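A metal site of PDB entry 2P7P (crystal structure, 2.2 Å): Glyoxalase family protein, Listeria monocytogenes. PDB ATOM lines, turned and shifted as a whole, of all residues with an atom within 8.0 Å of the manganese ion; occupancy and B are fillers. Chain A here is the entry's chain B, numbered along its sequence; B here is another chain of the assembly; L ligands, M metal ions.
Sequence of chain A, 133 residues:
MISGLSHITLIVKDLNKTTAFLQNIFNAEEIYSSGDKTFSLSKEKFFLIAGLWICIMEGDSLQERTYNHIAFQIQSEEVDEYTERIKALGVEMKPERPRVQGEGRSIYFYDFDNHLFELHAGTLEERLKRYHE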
ATOM      1  N   TYR A  67      13.287 -24.108 -21.420  1.00  0.00           N
ATOM      2  CA  TYR A  67      11.976 -23.566 -21.724  1.00  0.00           C
ATOM      3  C   TYR A  67      10.875 -24.102 -20.813  1.00  0.00           C
ATOM      4  O   TYR A  67       9.691 -23.895 -21.058  1.00  0.00           O
ATOM      5  CB  TYR A  67      11.630 -23.811 -23.197  1.00  0.00           C
ATOM      6  CG  TYR A  67      10.420 -23.025 -23.685  1.00  0.00           C
ATOM      7  CD1 TYR A  67      10.370 -21.636 -23.584  1.00  0.00           C
ATOM      8  CD2 TYR A  67       9.317 -23.680 -24.239  1.00  0.00           C
ATOM      9  CE1 TYR A  67       9.259 -20.911 -24.016  1.00  0.00           C
ATOM     10  CE2 TYR A  67       8.196 -22.968 -24.675  1.00  0.00           C
ATOM     11  CZ  TYR A  67       8.173 -21.581 -24.561  1.00  0.00           C
ATOM     12  OH  TYR A  67       7.066 -20.887 -24.998  1.00  0.00           O
ATOM     13  N   HIS A  69       8.539 -23.929 -17.840  1.00  0.00           N
ATOM     14  CA  HIS A  69       8.076 -22.737 -17.169  1.00  0.00           C
ATOM     15  C   HIS A  69       6.713 -22.833 -16.501  1.00  0.00           C
ATOM     16  O   HIS A  69       5.954 -23.781 -16.735  1.00  0.00           O
ATOM     17  CB  HIS A  69       8.082 -21.549 -18.151  1.00  0.00           C
ATOM     18  CG  HIS A  69       7.215 -21.741 -19.352  1.00  0.00           C
ATOM     19  ND1 HIS A  69       7.667 -22.328 -20.516  1.00  0.00           N
ATOM     20  CD2 HIS A  69       5.922 -21.403 -19.590  1.00  0.00           C
ATOM     21  CE1 HIS A  69       6.696 -22.339 -21.407  1.00  0.00           C
ATOM     22  NE2 HIS A  69       5.623 -21.783 -20.873  1.00  0.00           N
ATOM     23  N   ILE A  70       6.442 -21.836 -15.655  1.00  0.00           N
ATOM     24  CA  ILE A  70       5.181 -21.713 -14.936  1.00  0.00           C
ATOM     25  C   ILE A  70       4.558 -20.449 -15.469  1.00  0.00           C
ATOM     26  O   ILE A  70       5.235 -19.437 -15.625  1.00  0.00           O
ATOM     27  CB  ILE A  70       5.421 -21.551 -13.436  1.00  0.00           C
ATOM     28  CG1 ILE A  70       6.210 -22.742 -12.893  1.00  0.00           C
ATOM     29  CG2 ILE A  70       4.083 -21.402 -12.706  1.00  0.00           C
ATOM     30  CD1 ILE A  70       6.636 -22.586 -11.448  1.00  0.00           C
ATOM     31  N   ALA A  71       3.265 -20.495 -15.766  1.00  0.00           N
ATOM     32  CA  ALA A  71       2.579 -19.330 -16.307  1.00  0.00           C
ATOM     33  C   ALA A  71       1.365 -18.929 -15.487  1.00  0.00           C
ATOM     34  O   ALA A  71       0.552 -19.772 -15.106  1.00  0.00           O
ATOM     35  CB  ALA A  71       2.169 -19.605 -17.739  1.00  0.00           C
ATOM     36  N   PHE A  72       1.265 -17.638 -15.201  1.00  0.00           N
ATOM     37  CA  PHE A  72       0.132 -17.103 -14.444  1.00  0.00           C
ATOM     38  C   PHE A  72      -0.797 -16.364 -15.393  1.00  0.00           C
ATOM     39  O   PHE A  72      -0.379 -15.880 -16.448  1.00  0.00           O
ATOM     40  CB  PHE A  72       0.622 -16.175 -13.343  1.00  0.00           C
ATOM     41  CG  PHE A  72       1.417 -16.864 -12.271  1.00  0.00           C
ATOM     42  CD1 PHE A  72       2.788 -16.998 -12.373  1.00  0.00           C
ATOM     43  CD2 PHE A  72       0.772 -17.414 -11.161  1.00  0.00           C
ATOM     44  CE1 PHE A  72       3.518 -17.655 -11.394  1.00  0.00           C
ATOM     45  CE2 PHE A  72       1.486 -18.084 -10.173  1.00  0.00           C
ATOM     46  CZ  PHE A  72       2.870 -18.196 -10.285  1.00  0.00           C
ATOM     47  N   SER A 106       1.597 -13.152 -24.644  1.00  0.00           N
ATOM     48  CA  SER A 106       2.276 -13.675 -23.462  1.00  0.00           C
ATOM     49  C   SER A 106       3.568 -12.925 -23.185  1.00  0.00           C
ATOM     50  O   SER A 106       4.226 -12.434 -24.100  1.00  0.00           O
ATOM     51  CB  SER A 106       2.593 -15.158 -23.647  1.00  0.00           C
ATOM     52  OG  SER A 106       1.413 -15.934 -23.794  1.00  0.00           O
ATOM     53  N   ILE A 107       3.929 -12.842 -21.906  1.00  0.00           N
ATOM     54  CA  ILE A 107       5.158 -12.173 -21.521  1.00  0.00           C
ATOM     55  C   ILE A 107       6.073 -13.202 -20.867  1.00  0.00           C
ATOM     56  O   ILE A 107       5.671 -13.875 -19.913  1.00  0.00           O
ATOM     57  CB  ILE A 107       4.891 -11.045 -20.502  1.00  0.00           C
ATOM     58  CG1 ILE A 107       3.743 -10.159 -20.983  1.00  0.00           C
ATOM     59  CG2 ILE A 107       6.151 -10.214 -20.322  1.00  0.00           C
ATOM     60  CD1 ILE A 107       3.311  -9.124 -19.979  1.00  0.00           C
ATOM     61  N   TYR A 108       7.289 -13.312 -21.367  1.00  0.00           N
ATOM     62  CA  TYR A 108       8.262 -14.241 -20.824  1.00  0.00           C
ATOM     63  C   TYR A 108       9.408 -13.523 -20.138  1.00  0.00           C
ATOM     64  O   TYR A 108       9.914 -12.524 -20.642  1.00  0.00           O
ATOM     65  CB  TYR A 108       8.795 -15.164 -21.935  1.00  0.00           C
ATOM     66  CG  TYR A 108       7.769 -16.123 -22.485  1.00  0.00           C
ATOM     67  CD1 TYR A 108       7.008 -15.808 -23.608  1.00  0.00           C
ATOM     68  CD2 TYR A 108       7.538 -17.348 -21.860  1.00  0.00           C
ATOM     69  CE1 TYR A 108       6.033 -16.695 -24.107  1.00  0.00           C
ATOM     70  CE2 TYR A 108       6.572 -18.240 -22.339  1.00  0.00           C
ATOM     71  CZ  TYR A 108       5.818 -17.902 -23.460  1.00  0.00           C
ATOM     72  OH  TYR A 108       4.874 -18.788 -23.937  1.00  0.00           O
ATOM     73  N   LEU A 116      12.157 -19.694 -15.726  1.00  0.00           N
ATOM     74  CA  LEU A 116      11.402 -18.964 -16.735  1.00  0.00           C
ATOM     75  C   LEU A 116       9.934 -18.848 -16.342  1.00  0.00           C
ATOM     76  O   LEU A 116       9.258 -19.855 -16.156  1.00  0.00           O
ATOM     77  CB  LEU A 116      11.500 -19.645 -18.087  1.00  0.00           C
ATOM     78  CG  LEU A 116      10.580 -19.082 -19.170  1.00  0.00           C
ATOM     79  CD1 LEU A 116      11.015 -17.676 -19.564  1.00  0.00           C
ATOM     80  CD2 LEU A 116      10.600 -20.010 -20.389  1.00  0.00           C
ATOM     81  N   PHE A 117       9.452 -17.618 -16.188  1.00  0.00           N
ATOM     82  CA  PHE A 117       8.053 -17.390 -15.847  1.00  0.00           C
ATOM     83  C   PHE A 117       7.383 -16.774 -17.045  1.00  0.00           C
ATOM     84  O   PHE A 117       8.042 -16.238 -17.939  1.00  0.00           O
ATOM     85  CB  PHE A 117       7.895 -16.437 -14.661  1.00  0.00           C
ATOM     86  CG  PHE A 117       8.269 -17.022 -13.342  1.00  0.00           C
ATOM     87  CD1 PHE A 117       9.562 -16.881 -12.840  1.00  0.00           C
ATOM     88  CD2 PHE A 117       7.332 -17.731 -12.589  1.00  0.00           C
ATOM     89  CE1 PHE A 117       9.917 -17.420 -11.602  1.00  0.00           C
ATOM     90  CE2 PHE A 117       7.665 -18.275 -11.353  1.00  0.00           C
ATOM     91  CZ  PHE A 117       8.965 -18.123 -10.856  1.00  0.00           C
ATOM     92  N   GLU A 118       6.062 -16.820 -17.037  1.00  0.00           N
ATOM     93  CA  GLU A 118       5.275 -16.254 -18.114  1.00  0.00           C
ATOM     94  C   GLU A 118       4.007 -15.648 -17.555  1.00  0.00           C
ATOM     95  O   GLU A 118       3.456 -16.131 -16.560  1.00  0.00           O
ATOM     96  CB  GLU A 118       4.910 -17.344 -19.111  1.00  0.00           C
ATOM     97  CG  GLU A 118       4.105 -16.852 -20.295  1.00  0.00           C
ATOM     98  CD  GLU A 118       3.381 -17.983 -21.010  1.00  0.00           C
ATOM     99  OE1 GLU A 118       3.924 -19.103 -21.018  1.00  0.00           O
ATOM    100  OE2 GLU A 118       2.279 -17.752 -21.553  1.00  0.00           O
ATOM    101  N   LEU A 119       3.577 -14.558 -18.170  1.00  0.00           N
ATOM    102  CA  LEU A 119       2.337 -13.912 -17.794  1.00  0.00           C
ATOM    103  C   LEU A 119       1.494 -14.094 -19.038  1.00  0.00           C
ATOM    104  O   LEU A 119       1.801 -13.555 -20.100  1.00  0.00           O
ATOM    105  CB  LEU A 119       2.547 -12.436 -17.469  1.00  0.00           C
ATOM    106  CG  LEU A 119       3.191 -12.186 -16.094  1.00  0.00           C
ATOM    107  CD1 LEU A 119       3.290 -10.698 -15.852  1.00  0.00           C
ATOM    108  CD2 LEU A 119       2.359 -12.848 -15.008  1.00  0.00           C
ATOM    109  N   HIS A 120       0.452 -14.897 -18.911  1.00  0.00           N
ATOM    110  CA  HIS A 120      -0.384 -15.196 -20.053  1.00  0.00           C
ATOM    111  C   HIS A 120      -1.744 -14.516 -20.068  1.00  0.00           C
ATOM    112  O   HIS A 120      -2.493 -14.574 -19.106  1.00  0.00           O
ATOM    113  CB  HIS A 120      -0.561 -16.712 -20.151  1.00  0.00           C
ATOM    114  CG  HIS A 120      -1.305 -17.147 -21.368  1.00  0.00           C
ATOM    115  ND1 HIS A 120      -0.828 -16.955 -22.646  1.00  0.00           N
ATOM    116  CD2 HIS A 120      -2.513 -17.740 -21.506  1.00  0.00           C
ATOM    117  CE1 HIS A 120      -1.699 -17.418 -23.516  1.00  0.00           C
ATOM    118  NE2 HIS A 120      -2.732 -17.903 -22.849  1.00  0.00           N
ATOM    119  N   ARG A 127      -7.898 -20.675 -25.856  1.00  0.00           N
ATOM    120  CA  ARG A 127      -6.793 -21.384 -26.484  1.00  0.00           C
ATOM    121  C   ARG A 127      -7.255 -22.448 -27.496  1.00  0.00           C
ATOM    122  O   ARG A 127      -6.842 -22.429 -28.654  1.00  0.00           O
ATOM    123  CB  ARG A 127      -5.917 -22.044 -25.416  1.00  0.00           C
ATOM    124  CG  ARG A 127      -4.671 -22.708 -25.975  1.00  0.00           C
ATOM    125  CD  ARG A 127      -3.750 -21.682 -26.604  1.00  0.00           C
ATOM    126  NE  ARG A 127      -2.574 -22.296 -27.205  1.00  0.00           N
ATOM    127  CZ  ARG A 127      -1.557 -21.613 -27.718  1.00  0.00           C
ATOM    128  NH1 ARG A 127      -1.576 -20.283 -27.701  1.00  0.00           N
ATOM    129  NH2 ARG A 127      -0.522 -22.261 -28.249  1.00  0.00           N
ATOM    130  N   SER B   6      -2.137 -20.111 -15.012  1.00  0.00           N
ATOM    131  CA  SER B   6      -2.543 -20.346 -16.390  1.00  0.00           C
ATOM    132  C   SER B   6      -2.204 -21.782 -16.770  1.00  0.00           C
ATOM    133  O   SER B   6      -3.078 -22.547 -17.183  1.00  0.00           O
ATOM    134  CB  SER B   6      -1.811 -19.392 -17.326  1.00  0.00           C
ATOM    135  OG  SER B   6      -2.099 -19.699 -18.685  1.00  0.00           O
ATOM    136  N   HIS B   7      -0.933 -22.150 -16.625  1.00  0.00           N
ATOM    137  CA  HIS B   7      -0.501 -23.487 -16.976  1.00  0.00           C
ATOM    138  C   HIS B   7       0.964 -23.689 -16.604  1.00  0.00           C
ATOM    139  O   HIS B   7       1.646 -22.745 -16.210  1.00  0.00           O
ATOM    140  CB  HIS B   7      -0.672 -23.736 -18.479  1.00  0.00           C
ATOM    141  CG  HIS B   7       0.101 -22.783 -19.342  1.00  0.00           C
ATOM    142  ND1 HIS B   7      -0.353 -21.514 -19.643  1.00  0.00           N
ATOM    143  CD2 HIS B   7       1.290 -22.921 -19.977  1.00  0.00           C
ATOM    144  CE1 HIS B   7       0.527 -20.917 -20.424  1.00  0.00           C
ATOM    145  NE2 HIS B   7       1.525 -21.753 -20.644  1.00  0.00           N
ATOM    146  N   ILE B   8       1.418 -24.925 -16.747  1.00  0.00           N
ATOM    147  CA  ILE B   8       2.812 -25.287 -16.485  1.00  0.00           C
ATOM    148  C   ILE B   8       3.284 -26.038 -17.725  1.00  0.00           C
ATOM    149  O   ILE B   8       2.598 -26.936 -18.217  1.00  0.00           O
ATOM    150  CB  ILE B   8       2.933 -26.197 -15.257  1.00  0.00           C
ATOM    151  CG1 ILE B   8       2.526 -25.436 -13.987  1.00  0.00           C
ATOM    152  CG2 ILE B   8       4.363 -26.696 -15.126  1.00  0.00           C
ATOM    153  CD1 ILE B   8       2.509 -26.283 -12.747  1.00  0.00           C
ATOM    154  N   THR B   9       4.441 -25.654 -18.238  1.00  0.00           N
ATOM    155  CA  THR B   9       4.990 -26.272 -19.419  1.00  0.00           C
ATOM    156  C   THR B   9       6.282 -26.989 -19.076  1.00  0.00           C
ATOM    157  O   THR B   9       7.191 -26.390 -18.515  1.00  0.00           O
ATOM    158  CB  THR B   9       5.262 -25.225 -20.506  1.00  0.00           C
ATOM    159  OG1 THR B   9       4.021 -24.756 -21.047  1.00  0.00           O
ATOM    160  CG2 THR B   9       6.114 -25.813 -21.629  1.00  0.00           C
ATOM    161  N   PHE B  46      -1.326 -31.079 -24.641  1.00  0.00           N
ATOM    162  CA  PHE B  46      -1.850 -30.413 -23.459  1.00  0.00           C
ATOM    163  C   PHE B  46      -2.716 -31.380 -22.669  1.00  0.00           C
ATOM    164  O   PHE B  46      -3.514 -32.120 -23.235  1.00  0.00           O
ATOM    165  CB  PHE B  46      -2.669 -29.187 -23.869  1.00  0.00           C
ATOM    166  CG  PHE B  46      -1.875 -28.163 -24.649  1.00  0.00           C
ATOM    167  CD1 PHE B  46      -2.516 -27.107 -25.288  1.00  0.00           C
ATOM    168  CD2 PHE B  46      -0.482 -28.246 -24.727  1.00  0.00           C
ATOM    169  CE1 PHE B  46      -1.777 -26.158 -25.996  1.00  0.00           C
ATOM    170  CE2 PHE B  46       0.268 -27.305 -25.437  1.00  0.00           C
ATOM    171  CZ  PHE B  46      -0.382 -26.251 -26.073  1.00  0.00           C
ATOM    172  N   TRP B  53      -3.810 -27.010 -16.070  1.00  0.00           N
ATOM    173  CA  TRP B  53      -3.518 -27.105 -17.495  1.00  0.00           C
ATOM    174  C   TRP B  53      -2.018 -27.410 -17.623  1.00  0.00           C
ATOM    175  O   TRP B  53      -1.181 -26.535 -17.442  1.00  0.00           O
ATOM    176  CB  TRP B  53      -3.868 -25.764 -18.157  1.00  0.00           C
ATOM    177  CG  TRP B  53      -3.587 -25.651 -19.629  1.00  0.00           C
ATOM    178  CD1 TRP B  53      -3.319 -26.670 -20.489  1.00  0.00           C
ATOM    179  CD2 TRP B  53      -3.571 -24.440 -20.413  1.00  0.00           C
ATOM    180  NE1 TRP B  53      -3.136 -26.175 -21.769  1.00  0.00           N
ATOM    181  CE2 TRP B  53      -3.289 -24.813 -21.743  1.00  0.00           C
ATOM    182  CE3 TRP B  53      -3.766 -23.087 -20.119  1.00  0.00           C
ATOM    183  CZ2 TRP B  53      -3.197 -23.874 -22.783  1.00  0.00           C
ATOM    184  CZ3 TRP B  53      -3.681 -22.159 -21.153  1.00  0.00           C
ATOM    185  CH2 TRP B  53      -3.398 -22.561 -22.466  1.00  0.00           C
ATOM    186  N   CYS B  55       1.122 -28.601 -19.970  1.00  0.00           N
ATOM    187  CA  CYS B  55       1.563 -28.706 -21.358  1.00  0.00           C
ATOM    188  C   CYS B  55       2.906 -29.396 -21.444  1.00  0.00           C
ATOM    189  O   CYS B  55       3.802 -29.116 -20.647  1.00  0.00           O
ATOM    190  CB  CYS B  55       1.681 -27.323 -22.003  1.00  0.00           C
ATOM    191  SG  CYS B  55       0.134 -26.391 -22.045  1.00  0.00           S
ATOM    192  N   MET B  57       6.061 -30.416 -24.111  1.00  0.00           N
ATOM    193  CA  MET B  57       6.694 -30.125 -25.393  1.00  0.00           C
ATOM    194  C   MET B  57       7.909 -31.021 -25.535  1.00  0.00           C
ATOM    195  O   MET B  57       8.682 -31.183 -24.585  1.00  0.00           O
ATOM    196  CB  MET B  57       7.148 -28.676 -25.478  1.00  0.00           C
ATOM    197  CG  MET B  57       6.077 -27.678 -25.828  1.00  0.00           C
ATOM    198  SD  MET B  57       6.785 -26.003 -25.917  1.00  0.00           S
ATOM    199  CE  MET B  57       7.820 -26.145 -27.391  1.00  0.00           C
HETATM  200  S1  LIG L   1       2.698 -23.485 -24.199  1.00  0.00           S
HETATM  201  O1  LIG L   1       2.659 -23.072 -22.792  1.00  0.00           O
HETATM  202  O2  LIG L   1       2.515 -24.954 -24.263  1.00  0.00           O
HETATM  203  O3  LIG L   1       1.604 -22.836 -24.946  1.00  0.00           O
HETATM  204  O4  LIG L   1       3.988 -23.091 -24.784  1.00  0.00           O
HETATM  205 MN    MN M   1       3.339 -21.079 -21.891  1.00  0.00          MN
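N of Glu 118 is in hydrogen-bond range of O of Ile 70 (3.1 Å). OH of Tyr 67 sits at hydrogen-bond distance from OH of Tyr 108, 3.2 Å away. O of His 7 of chain B lies within hydrogen-bond range of N of Ala 71 (2.8 Å). ND1 of His 7 of chain B lies within hydrogen-bond range of OG of Ser 6 of chain B. ND1 of His 120 lies close to OE2 of Glu 118, 3.4 Å away. The side-chain hydroxyl (OG) of Ser 106 lies within hydrogen-bond range of the side-chain carboxylate (OE2) of Glu 118 (3.0 Å). The side-chain carboxylate (OE1) of Glu 118 sits close to the side-chain hydroxyl (OH) of Tyr 108 (3.1 Å). The backbone carbonyl oxygen (O) of Glu 118 sits at hydrogen-bond distance from the backbone NH (N) of Phe 72.
Merely in contact with the manganese ion: Tyr 108 (3.4 Å) and Thr 9 of chain B (3.8 Å).
The manganese ion is bound by OE1 of Glu 118, O1 of the ligand, NE2 of His 7 of chain B and NE2 of His 69.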
